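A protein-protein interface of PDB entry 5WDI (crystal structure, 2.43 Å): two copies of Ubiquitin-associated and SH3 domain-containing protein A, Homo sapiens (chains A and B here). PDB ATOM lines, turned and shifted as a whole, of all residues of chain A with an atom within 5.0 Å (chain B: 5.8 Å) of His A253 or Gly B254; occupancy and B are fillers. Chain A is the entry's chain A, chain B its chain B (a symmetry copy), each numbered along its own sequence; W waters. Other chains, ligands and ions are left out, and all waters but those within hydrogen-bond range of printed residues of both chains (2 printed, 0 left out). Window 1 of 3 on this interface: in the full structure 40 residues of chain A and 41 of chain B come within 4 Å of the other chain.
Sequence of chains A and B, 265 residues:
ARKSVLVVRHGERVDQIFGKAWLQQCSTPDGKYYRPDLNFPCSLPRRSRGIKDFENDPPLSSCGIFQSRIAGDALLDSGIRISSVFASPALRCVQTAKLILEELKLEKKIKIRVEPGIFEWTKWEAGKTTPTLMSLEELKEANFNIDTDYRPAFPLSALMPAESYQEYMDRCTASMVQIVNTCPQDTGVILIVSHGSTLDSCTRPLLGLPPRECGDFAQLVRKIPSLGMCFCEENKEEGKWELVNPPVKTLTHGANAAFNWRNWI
The backbone NH (N) of Asn B256 sits at hydrogen-bond distance from the backbone carbonyl oxygen (O) of His A253, at 3.0 Å. The backbone carbonyl oxygen of His B253 is in hydrogen-bond range of the backbone NH of Asn A256 (2.8 Å). O of Leu A251 lies within hydrogen-bond range of ND2 of Asn B256 (2.8 Å). ND2 of Asn B39 is in hydrogen-bond range of O of Thr A252 (2.8 Å). The side-chain sulfur of Cys B63 is in hydrogen-bond range of a ring nitrogen (ND1) of His A253 (3.6 Å). O of Gly B254 lies close to O of Gly A254 (3.5 Å). The side-chain hydroxyl of Thr A252 sits at hydrogen-bond distance from the side-chain carboxylate of Asp B37 (2.8 Å). The side-chain carboxylate (OE2) of Glu A12 sits at hydrogen-bond distance from the backbone NH (N) of Gly B254, at 2.8 Å. N of Gly A254 is in hydrogen-bond range of OE2 of Glu B12, 2.7 Å away.
OE1 of Glu B12 lies within hydrogen-bond range of OG of Ser B61 (2.5 Å). The backbone NH of Cys B63 sits close to the side-chain hydroxyl of Ser B61 (3.3 Å). The backbone NH (N) of Cys B63 sits at hydrogen-bond distance from the side-chain amide oxygen (OD1) of Asn B39, at 3.0 Å. The backbone NH (N) of Glu A12 sits at hydrogen-bond distance from the side-chain amide oxygen (OE1) of Gln A67, at 2.9 Å. A ring nitrogen (NE2) of His A253 is in hydrogen-bond range of the side-chain amide nitrogen (NE2) of Gln A67 (3.3 Å). OD1 of Asp B37 lies within hydrogen-bond range of N of Asn B39, at 2.9 Å.
Glu A12 touches His B253. CZ of Phe A66 touches N of Cys B63 (3.6 Å). Leu A251 touches Asn B39. Thr A252 touches Ile B17. Thr A252 touches Asn B256. His A253 touches Glu B12. O of His A253 touches CA of Ala B255 (3.5 Å). Gly A254 touches Ala B255 (C to CA, 3.9 Å). N of Ala B255 touches CB of Ala A255, at 3.8 Å. CA of Thr B252 touches O of Asn A256, at 3.2 Å.
Of the printed residues of chain B, Ile A17 touches Thr B252 and Gly B254. Of the printed residues of chain B, Phe A66 touches Cys B63. Gln A67 touches none of the printed residues of chain B. His A253 touches six residues of chain B. Gly B254 touches just these residues of chain A: Glu A12, Ile A17, His A253, Gly A254 and Ala A255. The nearest residue of chain A that does not touch Gly B254 is Cys A63 (4.6 Å). The nearest printed residue of chain A that does not touch Cys B63 is Gly A254 (4.4 Å).
Of the 11 printed residues of chain A, 10 touch a printed residue of chain B. Printed residues of chain A that touch a printed residue of chain B: Glu A12, Ile A17, Cys A63, Phe A66, Leu A251, Thr A252, His A253, Gly A254, Ala A255 and Asn A256. Hydrophobic or aromatic side chains of chain A within 4 Å of the printed part of chain B: Ile A17, Phe A66, Leu A251, His A253 and Ala A255. Hydrophobic or aromatic side chains of chain B that line the printed part of chain A: Ile B17, His B253 and Ala B255. Among the printed residues, 30 pairs touch across the chains. Among the printed residues, no Asp or Glu carboxylate lies within 4 Å of a Lys or Arg side-chain nitrogen of the other chain.
Glu A12 touches Gly B254, and with the chains exchanged Gly A254 touches Glu B12. Ile A17 touches Thr B252, and with the chains exchanged Thr A252 touches Ile B17. His A253 touches Asn B256, and with the chains exchanged Asn A256 touches His B253. Ala B255 touches its own counterpart, Ala A255.
Water W1 bridges N of Leu A251 (2.6 Å) and O of Ala B257 (3.0 Å). Water W2 lies within hydrogen-bond range of O of Ala B255 (2.9 Å), OD1 of Asn B256 (2.9 Å) and NE2 of Gln A67 (3.3 Å).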
ATOM      1  N   GLU A  12      14.233  12.882  -4.247  1.00  0.00           N
ATOM      2  CA  GLU A  12      15.195  13.947  -3.993  1.00  0.00           C
ATOM      3  C   GLU A  12      14.496  15.272  -3.719  1.00  0.00           C
ATOM      4  O   GLU A  12      13.660  15.719  -4.502  1.00  0.00           O
ATOM      5  CB  GLU A  12      16.138  14.116  -5.186  1.00  0.00           C
ATOM      6  CG  GLU A  12      17.249  15.129  -4.951  1.00  0.00           C
ATOM      7  CD  GLU A  12      18.096  15.391  -6.182  1.00  0.00           C
ATOM      8  OE1 GLU A  12      17.728  16.242  -7.021  1.00  0.00           O
ATOM      9  OE2 GLU A  12      19.151  14.754  -6.296  1.00  0.00           O
ATOM     10  N   ILE A  17      20.359  19.168  -2.585  1.00  0.00           N
ATOM     11  CA  ILE A  17      21.331  19.545  -3.613  1.00  0.00           C
ATOM     12  C   ILE A  17      21.757  20.996  -3.484  1.00  0.00           C
ATOM     13  O   ILE A  17      22.947  21.299  -3.548  1.00  0.00           O
ATOM     14  CB  ILE A  17      20.753  19.338  -5.036  1.00  0.00           C
ATOM     15  CG1 ILE A  17      20.282  17.892  -5.223  1.00  0.00           C
ATOM     16  CG2 ILE A  17      21.773  19.699  -6.108  1.00  0.00           C
ATOM     17  CD1 ILE A  17      21.338  16.846  -4.931  1.00  0.00           C
ATOM     18  N   CYS A  63      14.710  16.066 -10.406  1.00  0.00           N
ATOM     19  CA  CYS A  63      15.172  14.683 -10.303  1.00  0.00           C
ATOM     20  C   CYS A  63      14.254  13.848  -9.403  1.00  0.00           C
ATOM     21  O   CYS A  63      13.900  12.720  -9.740  1.00  0.00           O
ATOM     22  CB  CYS A  63      16.599  14.621  -9.773  1.00  0.00           C
ATOM     23  SG  CYS A  63      17.340  12.987  -9.968  1.00  0.00           S
ATOM     24  N   PHE A  66      11.328  12.843 -11.259  1.00  0.00           N
ATOM     25  CA  PHE A  66      11.691  11.724 -12.142  1.00  0.00           C
ATOM     26  C   PHE A  66      11.720  10.391 -11.390  1.00  0.00           C
ATOM     27  O   PHE A  66      11.187   9.390 -11.867  1.00  0.00           O
ATOM     28  CB  PHE A  66      13.035  11.991 -12.830  1.00  0.00           C
ATOM     29  CG  PHE A  66      13.828  10.753 -13.122  1.00  0.00           C
ATOM     30  CD1 PHE A  66      13.399   9.847 -14.089  1.00  0.00           C
ATOM     31  CD2 PHE A  66      15.022  10.501 -12.448  1.00  0.00           C
ATOM     32  CE1 PHE A  66      14.134   8.702 -14.363  1.00  0.00           C
ATOM     33  CE2 PHE A  66      15.756   9.357 -12.716  1.00  0.00           C
ATOM     34  CZ  PHE A  66      15.315   8.459 -13.676  1.00  0.00           C
ATOM     35  N   GLN A  67      12.332  10.390 -10.214  1.00  0.00           N
ATOM     36  CA  GLN A  67      12.459   9.180  -9.414  1.00  0.00           C
ATOM     37  C   GLN A  67      11.076   8.669  -9.006  1.00  0.00           C
ATOM     38  O   GLN A  67      10.779   7.480  -9.142  1.00  0.00           O
ATOM     39  CB  GLN A  67      13.292   9.456  -8.166  1.00  0.00           C
ATOM     40  CG  GLN A  67      14.743   9.851  -8.420  1.00  0.00           C
ATOM     41  CD  GLN A  67      15.397  10.470  -7.196  1.00  0.00           C
ATOM     42  OE1 GLN A  67      14.721  10.878  -6.263  1.00  0.00           O
ATOM     43  NE2 GLN A  67      16.715  10.544  -7.201  1.00  0.00           N
ATOM     44  N   LEU A 251      16.692   1.687  -7.806  1.00  0.00           N
ATOM     45  CA  LEU A 251      16.935   2.731  -8.797  1.00  0.00           C
ATOM     46  C   LEU A 251      18.292   3.371  -8.556  1.00  0.00           C
ATOM     47  O   LEU A 251      18.470   4.122  -7.589  1.00  0.00           O
ATOM     48  CB  LEU A 251      15.844   3.799  -8.749  1.00  0.00           C
ATOM     49  CG  LEU A 251      16.109   5.038  -9.621  1.00  0.00           C
ATOM     50  CD1 LEU A 251      16.237   4.675 -11.093  1.00  0.00           C
ATOM     51  CD2 LEU A 251      15.028   6.084  -9.424  1.00  0.00           C
ATOM     52  N   THR A 252      19.235   3.093  -9.451  1.00  0.00           N
ATOM     53  CA  THR A 252      20.632   3.470  -9.254  1.00  0.00           C
ATOM     54  C   THR A 252      21.106   4.329 -10.412  1.00  0.00           C
ATOM     55  O   THR A 252      21.163   3.856 -11.547  1.00  0.00           O
ATOM     56  CB  THR A 252      21.525   2.211  -9.159  1.00  0.00           C
ATOM     57  OG1 THR A 252      20.996   1.331  -8.157  1.00  0.00           O
ATOM     58  CG2 THR A 252      22.976   2.586  -8.817  1.00  0.00           C
ATOM     59  N   HIS A 253      21.452   5.586 -10.123  1.00  0.00           N
ATOM     60  CA  HIS A 253      21.951   6.499 -11.148  1.00  0.00           C
ATOM     61  C   HIS A 253      22.989   7.495 -10.636  1.00  0.00           C
ATOM     62  O   HIS A 253      23.160   7.671  -9.431  1.00  0.00           O
ATOM     63  CB  HIS A 253      20.789   7.247 -11.805  1.00  0.00           C
ATOM     64  CG  HIS A 253      20.047   8.164 -10.885  1.00  0.00           C
ATOM     65  ND1 HIS A 253      20.468   9.444 -10.608  1.00  0.00           N
ATOM     66  CD2 HIS A 253      18.889   7.997 -10.209  1.00  0.00           C
ATOM     67  CE1 HIS A 253      19.611  10.018  -9.784  1.00  0.00           C
ATOM     68  NE2 HIS A 253      18.641   9.162  -9.532  1.00  0.00           N
ATOM     69  N   GLY A 254      23.663   8.151 -11.578  1.00  0.00           N
ATOM     70  CA  GLY A 254      24.728   9.096 -11.269  1.00  0.00           C
ATOM     71  C   GLY A 254      24.217  10.488 -10.946  1.00  0.00           C
ATOM     72  O   GLY A 254      23.055  10.808 -11.162  1.00  0.00           O
ATOM     73  N   ALA A 255      25.100  11.307 -10.397  1.00  0.00           N
ATOM     74  CA  ALA A 255      24.822  12.717 -10.170  1.00  0.00           C
ATOM     75  C   ALA A 255      25.010  13.478 -11.470  1.00  0.00           C
ATOM     76  O   ALA A 255      25.378  12.896 -12.489  1.00  0.00           O
ATOM     77  CB  ALA A 255      25.758  13.265  -9.101  1.00  0.00           C
ATOM     78  N   ASN A 256      24.747  14.773 -11.438  1.00  0.00           N
ATOM     79  CA  ASN A 256      25.077  15.644 -12.552  1.00  0.00           C
ATOM     80  C   ASN A 256      25.544  16.988 -12.018  1.00  0.00           C
ATOM     81  O   ASN A 256      24.795  17.690 -11.354  1.00  0.00           O
ATOM     82  CB  ASN A 256      23.880  15.813 -13.493  1.00  0.00           C
ATOM     83  CG  ASN A 256      24.305  16.056 -14.935  1.00  0.00           C
ATOM     84  OD1 ASN A 256      25.122  15.309 -15.481  1.00  0.00           O
ATOM     85  ND2 ASN A 256      23.755  17.099 -15.563  1.00  0.00           N
ATOM     86  N   GLU B  12      23.034  10.622 -19.546  1.00  0.00           N
ATOM     87  CA  GLU B  12      23.679   9.495 -18.882  1.00  0.00           C
ATOM     88  C   GLU B  12      23.516   8.189 -19.659  1.00  0.00           C
ATOM     89  O   GLU B  12      22.404   7.778 -19.974  1.00  0.00           O
ATOM     90  CB  GLU B  12      23.125   9.320 -17.458  1.00  0.00           C
ATOM     91  CG  GLU B  12      23.818   8.244 -16.635  1.00  0.00           C
ATOM     92  CD  GLU B  12      23.164   8.009 -15.286  1.00  0.00           C
ATOM     93  OE1 GLU B  12      22.166   7.270 -15.233  1.00  0.00           O
ATOM     94  OE2 GLU B  12      23.671   8.532 -14.266  1.00  0.00           O
ATOM     95  N   ILE B  17      27.196   3.792 -15.168  1.00  0.00           N
ATOM     96  CA  ILE B  17      26.721   3.384 -13.857  1.00  0.00           C
ATOM     97  C   ILE B  17      26.925   1.898 -13.618  1.00  0.00           C
ATOM     98  O   ILE B  17      27.322   1.492 -12.527  1.00  0.00           O
ATOM     99  CB  ILE B  17      25.223   3.692 -13.715  1.00  0.00           C
ATOM    100  CG1 ILE B  17      24.961   5.175 -14.005  1.00  0.00           C
ATOM    101  CG2 ILE B  17      24.720   3.306 -12.331  1.00  0.00           C
ATOM    102  CD1 ILE B  17      25.833   6.130 -13.211  1.00  0.00           C
ATOM    103  N   ASP B  37      17.692  -3.282 -12.619  1.00  0.00           N
ATOM    104  CA  ASP B  37      17.563  -2.039 -11.848  1.00  0.00           C
ATOM    105  C   ASP B  37      16.702  -1.115 -12.701  1.00  0.00           C
ATOM    106  O   ASP B  37      16.724  -1.214 -13.923  1.00  0.00           O
ATOM    107  CB  ASP B  37      18.960  -1.442 -11.615  1.00  0.00           C
ATOM    108  CG  ASP B  37      18.952  -0.201 -10.729  1.00  0.00           C
ATOM    109  OD1 ASP B  37      18.691   0.913 -11.240  1.00  0.00           O
ATOM    110  OD2 ASP B  37      19.258  -0.330  -9.521  1.00  0.00           O
ATOM    111  N   ASN B  39      17.040   1.905 -13.457  1.00  0.00           N
ATOM    112  CA  ASN B  39      17.792   2.822 -14.292  1.00  0.00           C
ATOM    113  C   ASN B  39      18.184   2.223 -15.649  1.00  0.00           C
ATOM    114  O   ASN B  39      18.678   2.935 -16.530  1.00  0.00           O
ATOM    115  CB  ASN B  39      19.034   3.322 -13.568  1.00  0.00           C
ATOM    116  CG  ASN B  39      19.566   4.596 -14.171  1.00  0.00           C
ATOM    117  OD1 ASN B  39      18.800   5.435 -14.653  1.00  0.00           O
ATOM    118  ND2 ASN B  39      20.875   4.754 -14.157  1.00  0.00           N
ATOM    119  N   SER B  61      20.527   5.707 -19.939  1.00  0.00           N
ATOM    120  CA  SER B  61      19.882   5.213 -18.730  1.00  0.00           C
ATOM    121  C   SER B  61      18.535   5.894 -18.608  1.00  0.00           C
ATOM    122  O   SER B  61      18.242   6.827 -19.344  1.00  0.00           O
ATOM    123  CB  SER B  61      20.727   5.544 -17.505  1.00  0.00           C
ATOM    124  OG  SER B  61      20.784   6.945 -17.296  1.00  0.00           O
ATOM    125  N   CYS B  63      17.777   7.810 -16.239  1.00  0.00           N
ATOM    126  CA  CYS B  63      18.200   9.143 -15.827  1.00  0.00           C
ATOM    127  C   CYS B  63      18.580   9.965 -17.050  1.00  0.00           C
ATOM    128  O   CYS B  63      18.229  11.137 -17.152  1.00  0.00           O
ATOM    129  CB  CYS B  63      19.378   9.037 -14.860  1.00  0.00           C
ATOM    130  SG  CYS B  63      19.673  10.533 -13.904  1.00  0.00           S
ATOM    131  N   THR B 252      21.618  20.381 -12.267  1.00  0.00           N
ATOM    132  CA  THR B 252      22.441  19.866 -11.185  1.00  0.00           C
ATOM    133  C   THR B 252      21.583  18.987 -10.299  1.00  0.00           C
ATOM    134  O   THR B 252      20.618  19.468  -9.708  1.00  0.00           O
ATOM    135  CB  THR B 252      23.017  21.015 -10.331  1.00  0.00           C
ATOM    136  OG1 THR B 252      23.566  22.026 -11.186  1.00  0.00           O
ATOM    137  CG2 THR B 252      24.089  20.505  -9.400  1.00  0.00           C
ATOM    138  N   HIS B 253      21.928  17.706 -10.202  1.00  0.00           N
ATOM    139  CA  HIS B 253      21.214  16.793  -9.303  1.00  0.00           C
ATOM    140  C   HIS B 253      22.119  15.724  -8.721  1.00  0.00           C
ATOM    141  O   HIS B 253      23.219  15.474  -9.217  1.00  0.00           O
ATOM    142  CB  HIS B 253      20.025  16.144 -10.006  1.00  0.00           C
ATOM    143  CG  HIS B 253      20.401  15.253 -11.149  1.00  0.00           C
ATOM    144  ND1 HIS B 253      21.034  14.039 -10.979  1.00  0.00           N
ATOM    145  CD2 HIS B 253      20.197  15.386 -12.481  1.00  0.00           C
ATOM    146  CE1 HIS B 253      21.216  13.470 -12.158  1.00  0.00           C
ATOM    147  NE2 HIS B 253      20.716  14.267 -13.085  1.00  0.00           N
ATOM    148  N   GLY B 254      21.630  15.094  -7.659  1.00  0.00           N
ATOM    149  CA  GLY B 254      22.408  14.123  -6.912  1.00  0.00           C
ATOM    150  C   GLY B 254      22.331  12.725  -7.487  1.00  0.00           C
ATOM    151  O   GLY B 254      21.638  12.479  -8.467  1.00  0.00           O
ATOM    152  N   ALA B 255      23.058  11.819  -6.854  1.00  0.00           N
ATOM    153  CA  ALA B 255      23.058  10.409  -7.201  1.00  0.00           C
ATOM    154  C   ALA B 255      21.979   9.661  -6.436  1.00  0.00           C
ATOM    155  O   ALA B 255      21.358  10.206  -5.539  1.00  0.00           O
ATOM    156  CB  ALA B 255      24.419   9.800  -6.891  1.00  0.00           C
ATOM    157  N   ASN B 256      21.758   8.413  -6.828  1.00  0.00           N
ATOM    158  CA  ASN B 256      20.912   7.490  -6.089  1.00  0.00           C
ATOM    159  C   ASN B 256      21.621   6.139  -6.020  1.00  0.00           C
ATOM    160  O   ASN B 256      22.047   5.595  -7.043  1.00  0.00           O
ATOM    161  CB  ASN B 256      19.531   7.352  -6.747  1.00  0.00           C
ATOM    162  CG  ASN B 256      18.414   7.123  -5.733  1.00  0.00           C
ATOM    163  OD1 ASN B 256      18.350   7.802  -4.713  1.00  0.00           O
ATOM    164  ND2 ASN B 256      17.529   6.172  -6.012  1.00  0.00           N
ATOM    165  N   ALA B 257      21.769   5.621  -4.809  1.00  0.00           N
ATOM    166  CA  ALA B 257      22.460   4.362  -4.590  1.00  0.00           C
ATOM    167  C   ALA B 257      21.447   3.223  -4.534  1.00  0.00           C
ATOM    168  O   ALA B 257      20.254   3.445  -4.340  1.00  0.00           O
ATOM    169  CB  ALA B 257      23.261   4.428  -3.303  1.00  0.00           C
HETATM  170  O   HOH W   1      17.723   2.249  -5.485  1.00  0.00           O
HETATM  171  O   HOH W   2      18.711  10.686  -4.549  1.00  0.00           O
